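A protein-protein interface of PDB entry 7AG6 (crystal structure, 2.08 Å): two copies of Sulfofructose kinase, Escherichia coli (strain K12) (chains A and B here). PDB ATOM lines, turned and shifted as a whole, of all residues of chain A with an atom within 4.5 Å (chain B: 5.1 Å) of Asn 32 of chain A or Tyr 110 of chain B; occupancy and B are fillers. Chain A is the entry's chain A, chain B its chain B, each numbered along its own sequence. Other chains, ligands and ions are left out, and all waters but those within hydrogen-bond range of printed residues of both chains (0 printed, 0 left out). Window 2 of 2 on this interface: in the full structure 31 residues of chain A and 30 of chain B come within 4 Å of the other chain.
The side-chain amide oxygen (OE1) of Gln 94 of chain B lies within hydrogen-bond range of the side-chain hydroxyl (OH) of Tyr 16 of chain A. O of Asn 109 of chain B lies within hydrogen-bond range of N of Ala 30 of chain A (2.8 Å).
N of Tyr 17 of chain A lies within hydrogen-bond range of O of Asn 32 of chain A, at 2.9 Å. O of Gln 94 of chain B sits at hydrogen-bond distance from ND2 of Asn 109 of chain B (3.3 Å). The backbone NH of Tyr 110 of chain B lies within hydrogen-bond range of the backbone carbonyl oxygen of Gln 94 of chain B (2.9 Å). OG of Ser 95 of chain B lies within hydrogen-bond range of ND2 of Asn 109 of chain B (2.9 Å).
Ser 95 of chain B touches Tyr 16 of chain A (C to OH, 3.9 Å). Tyr 16 of chain A touches Ile 108 of chain B. O of Ala 30 of chain A touches CD1 of Tyr 110 of chain B, 3.99 Å away. CE1 of Tyr 110 of chain B touches CA of Asn 32 of chain A, 3.8 Å away. CE1 of Tyr 33 of chain A touches NE2 of Gln 94 of chain B, at 3.6 Å. Tyr 110 of chain B touches Tyr 33 of chain A.
Printed residues of chain A within 4 Å of Tyr 110 of chain B: Ala 30, Asn 32 and Tyr 33. Printed residues of chain A within 4 Å of Ser 95 of chain B: Tyr 16. Printed residues of chain A within 4 Å of Gln 94 of chain B: Tyr 16 and Tyr 33. Printed residues of chain B within 4 Å of Ala 30 of chain A: Asn 109 (2.8 Å) and Tyr 110 (3.99 Å). Ile 15 of chain A touches none of the printed residues of chain B. The nearest printed residue of chain B that does not touch Asn 32 of chain A is Pro 113 of chain B (6.8 Å). The nearest printed residue of chain B that does not touch Tyr 33 of chain A is Pro 111 of chain B (7.2 Å).
Of the 9 printed residues of chain B, 5 touch a printed residue of chain A. Hydrophobic or aromatic side chains of chain B within 4 Å of the printed part of chain A: Ile 108 and Tyr 110. Of the 7 printed residues of chain A, 4 touch a printed residue of chain B. Among the printed residues, 8 pairs touch across the chains.
No position is printed for both chains. Of the 8 pairs that touch across the chains among the printed residues, none has its exchanged pair printed and touching as well.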
ATOM      1  N   ILE A  15      34.652  13.360   0.046  1.00  0.00           N
ATOM      2  CA  ILE A  15      34.620  14.058   1.362  1.00  0.00           C
ATOM      3  C   ILE A  15      33.286  14.808   1.521  1.00  0.00           C
ATOM      4  O   ILE A  15      32.999  15.712   0.734  1.00  0.00           O
ATOM      5  CB  ILE A  15      35.843  14.976   1.541  1.00  0.00           C
ATOM      6  CG1 ILE A  15      37.134  14.323   1.053  1.00  0.00           C
ATOM      7  CG2 ILE A  15      35.933  15.410   2.994  1.00  0.00           C
ATOM      8  CD1 ILE A  15      38.369  15.183   1.202  1.00  0.00           C
ATOM      9  N   TYR A  16      32.539  14.424   2.550  1.00  0.00           N
ATOM     10  CA  TYR A  16      31.235  14.961   2.965  1.00  0.00           C
ATOM     11  C   TYR A  16      31.475  15.826   4.206  1.00  0.00           C
ATOM     12  O   TYR A  16      31.932  15.304   5.240  1.00  0.00           O
ATOM     13  CB  TYR A  16      30.277  13.793   3.218  1.00  0.00           C
ATOM     14  CG  TYR A  16      30.006  12.926   2.003  1.00  0.00           C
ATOM     15  CD1 TYR A  16      30.900  11.936   1.632  1.00  0.00           C
ATOM     16  CD2 TYR A  16      28.870  13.084   1.220  1.00  0.00           C
ATOM     17  CE1 TYR A  16      30.689  11.139   0.526  1.00  0.00           C
ATOM     18  CE2 TYR A  16      28.633  12.282   0.106  1.00  0.00           C
ATOM     19  CZ  TYR A  16      29.543  11.292  -0.228  1.00  0.00           C
ATOM     20  OH  TYR A  16      29.403  10.467  -1.300  1.00  0.00           O
ATOM     21  N   TYR A  17      31.194  17.119   4.106  1.00  0.00           N
ATOM     22  CA  TYR A  17      31.251  18.073   5.240  1.00  0.00           C
ATOM     23  C   TYR A  17      29.882  18.082   5.893  1.00  0.00           C
ATOM     24  O   TYR A  17      28.913  18.493   5.231  1.00  0.00           O
ATOM     25  CB  TYR A  17      31.707  19.448   4.752  1.00  0.00           C
ATOM     26  CG  TYR A  17      33.107  19.378   4.212  1.00  0.00           C
ATOM     27  CD1 TYR A  17      34.195  19.513   5.064  1.00  0.00           C
ATOM     28  CD2 TYR A  17      33.342  18.991   2.902  1.00  0.00           C
ATOM     29  CE1 TYR A  17      35.489  19.331   4.609  1.00  0.00           C
ATOM     30  CE2 TYR A  17      34.634  18.847   2.430  1.00  0.00           C
ATOM     31  CZ  TYR A  17      35.712  19.004   3.286  1.00  0.00           C
ATOM     32  OH  TYR A  17      36.998  18.838   2.844  1.00  0.00           O
ATOM     33  N   ALA A  30      24.852  16.334   3.946  1.00  0.00           N
ATOM     34  CA  ALA A  30      26.136  17.058   3.859  1.00  0.00           C
ATOM     35  C   ALA A  30      25.861  18.508   3.443  1.00  0.00           C
ATOM     36  O   ALA A  30      25.064  18.700   2.511  1.00  0.00           O
ATOM     37  CB  ALA A  30      27.025  16.371   2.863  1.00  0.00           C
ATOM     38  N   ARG A  31      26.518  19.462   4.082  1.00  0.00           N
ATOM     39  CA  ARG A  31      26.519  20.907   3.721  1.00  0.00           C
ATOM     40  C   ARG A  31      27.382  21.124   2.488  1.00  0.00           C
ATOM     41  O   ARG A  31      27.246  22.145   1.828  1.00  0.00           O
ATOM     42  CB  ARG A  31      27.157  21.768   4.814  1.00  0.00           C
ATOM     43  CG  ARG A  31      26.388  21.830   6.121  1.00  0.00           C
ATOM     44  CD  ARG A  31      27.443  22.015   7.168  1.00  0.00           C
ATOM     45  NE  ARG A  31      26.919  22.530   8.415  1.00  0.00           N
ATOM     46  CZ  ARG A  31      27.570  23.405   9.168  1.00  0.00           C
ATOM     47  NH1 ARG A  31      28.743  23.885   8.773  1.00  0.00           N
ATOM     48  NH2 ARG A  31      27.035  23.810  10.306  1.00  0.00           N
ATOM     49  N   ASN A  32      28.332  20.241   2.250  1.00  0.00           N
ATOM     50  CA  ASN A  32      29.287  20.435   1.137  1.00  0.00           C
ATOM     51  C   ASN A  32      29.982  19.109   0.841  1.00  0.00           C
ATOM     52  O   ASN A  32      29.905  18.182   1.678  1.00  0.00           O
ATOM     53  CB  ASN A  32      30.318  21.498   1.510  1.00  0.00           C
ATOM     54  CG  ASN A  32      30.821  22.270   0.317  1.00  0.00           C
ATOM     55  OD1 ASN A  32      30.705  21.843  -0.842  1.00  0.00           O
ATOM     56  ND2 ASN A  32      31.361  23.426   0.609  1.00  0.00           N
ATOM     57  N   TYR A  33      30.644  19.038  -0.308  1.00  0.00           N
ATOM     58  CA  TYR A  33      31.211  17.787  -0.851  1.00  0.00           C
ATOM     59  C   TYR A  33      32.389  18.152  -1.734  1.00  0.00           C
ATOM     60  O   TYR A  33      32.296  19.078  -2.537  1.00  0.00           O
ATOM     61  CB  TYR A  33      30.178  16.981  -1.638  1.00  0.00           C
ATOM     62  CG  TYR A  33      30.767  15.785  -2.340  1.00  0.00           C
ATOM     63  CD1 TYR A  33      31.041  14.620  -1.643  1.00  0.00           C
ATOM     64  CD2 TYR A  33      31.124  15.840  -3.683  1.00  0.00           C
ATOM     65  CE1 TYR A  33      31.668  13.550  -2.256  1.00  0.00           C
ATOM     66  CE2 TYR A  33      31.729  14.770  -4.318  1.00  0.00           C
ATOM     67  CZ  TYR A  33      31.983  13.608  -3.602  1.00  0.00           C
ATOM     68  OH  TYR A  33      32.588  12.530  -4.184  1.00  0.00           O
ATOM     69  N   SER B  93      22.955  14.095  -7.861  1.00  0.00           N
ATOM     70  CA  SER B  93      23.055  13.904  -6.402  1.00  0.00           C
ATOM     71  C   SER B  93      23.588  12.495  -6.119  1.00  0.00           C
ATOM     72  O   SER B  93      23.413  11.600  -6.960  1.00  0.00           O
ATOM     73  CB  SER B  93      21.714  14.126  -5.758  1.00  0.00           C
ATOM     74  OG  SER B  93      21.305  15.472  -5.908  1.00  0.00           O
ATOM     75  N   GLN B  94      24.186  12.298  -4.950  1.00  0.00           N
ATOM     76  CA  GLN B  94      24.700  10.979  -4.526  1.00  0.00           C
ATOM     77  C   GLN B  94      24.721  10.919  -2.996  1.00  0.00           C
ATOM     78  O   GLN B  94      24.633  11.958  -2.346  1.00  0.00           O
ATOM     79  CB  GLN B  94      26.050  10.688  -5.212  1.00  0.00           C
ATOM     80  CG  GLN B  94      27.070  11.828  -5.196  1.00  0.00           C
ATOM     81  CD  GLN B  94      27.750  11.996  -3.855  1.00  0.00           C
ATOM     82  OE1 GLN B  94      27.677  11.142  -2.963  1.00  0.00           O
ATOM     83  NE2 GLN B  94      28.437  13.105  -3.709  1.00  0.00           N
ATOM     84  N   SER B  95      24.820   9.707  -2.458  1.00  0.00           N
ATOM     85  CA  SER B  95      24.885   9.420  -1.009  1.00  0.00           C
ATOM     86  C   SER B  95      26.057   8.477  -0.740  1.00  0.00           C
ATOM     87  O   SER B  95      26.363   7.613  -1.589  1.00  0.00           O
ATOM     88  CB  SER B  95      23.621   8.790  -0.527  1.00  0.00           C
ATOM     89  OG  SER B  95      22.528   9.667  -0.660  1.00  0.00           O
ATOM     90  N   ILE B 108      24.582   9.445   4.338  1.00  0.00           N
ATOM     91  CA  ILE B 108      24.992  10.864   4.172  1.00  0.00           C
ATOM     92  C   ILE B 108      24.611  11.245   2.751  1.00  0.00           C
ATOM     93  O   ILE B 108      25.257  10.719   1.830  1.00  0.00           O
ATOM     94  CB  ILE B 108      26.507  11.065   4.396  1.00  0.00           C
ATOM     95  CG1 ILE B 108      27.046  10.302   5.605  1.00  0.00           C
ATOM     96  CG2 ILE B 108      26.812  12.547   4.456  1.00  0.00           C
ATOM     97  CD1 ILE B 108      26.453  10.745   6.910  1.00  0.00           C
ATOM     98  N   ASN B 109      23.583  12.069   2.583  1.00  0.00           N
ATOM     99  CA  ASN B 109      23.158  12.523   1.235  1.00  0.00           C
ATOM    100  C   ASN B 109      23.800  13.876   0.930  1.00  0.00           C
ATOM    101  O   ASN B 109      23.850  14.730   1.828  1.00  0.00           O
ATOM    102  CB  ASN B 109      21.641  12.580   1.076  1.00  0.00           C
ATOM    103  CG  ASN B 109      21.247  13.089  -0.295  1.00  0.00           C
ATOM    104  OD1 ASN B 109      20.710  14.179  -0.415  1.00  0.00           O
ATOM    105  ND2 ASN B 109      21.560  12.333  -1.334  1.00  0.00           N
ATOM    106  N   TYR B 110      24.283  14.041  -0.298  1.00  0.00           N
ATOM    107  CA  TYR B 110      24.756  15.332  -0.850  1.00  0.00           C
ATOM    108  C   TYR B 110      23.851  15.720  -2.016  1.00  0.00           C
ATOM    109  O   TYR B 110      23.978  15.210  -3.138  1.00  0.00           O
ATOM    110  CB  TYR B 110      26.217  15.299  -1.300  1.00  0.00           C
ATOM    111  CG  TYR B 110      26.653  16.629  -1.848  1.00  0.00           C
ATOM    112  CD1 TYR B 110      26.632  17.747  -1.037  1.00  0.00           C
ATOM    113  CD2 TYR B 110      26.952  16.805  -3.186  1.00  0.00           C
ATOM    114  CE1 TYR B 110      26.975  19.000  -1.518  1.00  0.00           C
ATOM    115  CE2 TYR B 110      27.276  18.054  -3.693  1.00  0.00           C
ATOM    116  CZ  TYR B 110      27.323  19.146  -2.845  1.00  0.00           C
ATOM    117  OH  TYR B 110      27.615  20.393  -3.315  1.00  0.00           O
ATOM    118  N   PRO B 111      22.893  16.636  -1.764  1.00  0.00           N
ATOM    119  CA  PRO B 111      22.015  17.133  -2.818  1.00  0.00           C
ATOM    120  C   PRO B 111      22.812  18.097  -3.701  1.00  0.00           C
ATOM    121  O   PRO B 111      23.401  19.017  -3.170  1.00  0.00           O
ATOM    122  CB  PRO B 111      20.857  17.810  -2.070  1.00  0.00           C
ATOM    123  CG  PRO B 111      21.378  18.089  -0.684  1.00  0.00           C
ATOM    124  CD  PRO B 111      22.585  17.205  -0.450  1.00  0.00           C
ATOM    125  N   SER B 112      22.907  17.787  -4.992  1.00  0.00           N
ATOM    126  CA  SER B 112      23.635  18.611  -5.987  1.00  0.00           C
ATOM    127  C   SER B 112      23.073  20.032  -5.941  1.00  0.00           C
ATOM    128  O   SER B 112      21.877  20.214  -6.106  1.00  0.00           O
ATOM    129  CB  SER B 112      23.518  18.050  -7.382  1.00  0.00           C
ATOM    130  OG  SER B 112      23.986  19.001  -8.348  1.00  0.00           O
ATOM    131  N   PRO B 113      23.913  21.074  -5.819  1.00  0.00           N
ATOM    132  CA  PRO B 113      23.445  22.454  -5.970  1.00  0.00           C
ATOM    133  C   PRO B 113      23.117  22.863  -7.418  1.00  0.00           C
ATOM    134  O   PRO B 113      22.625  23.993  -7.615  1.00  0.00           O
ATOM    135  CB  PRO B 113      24.600  23.287  -5.404  1.00  0.00           C
ATOM    136  CG  PRO B 113      25.856  22.408  -5.536  1.00  0.00           C
ATOM    137  CD  PRO B 113      25.350  20.979  -5.561  1.00  0.00           C
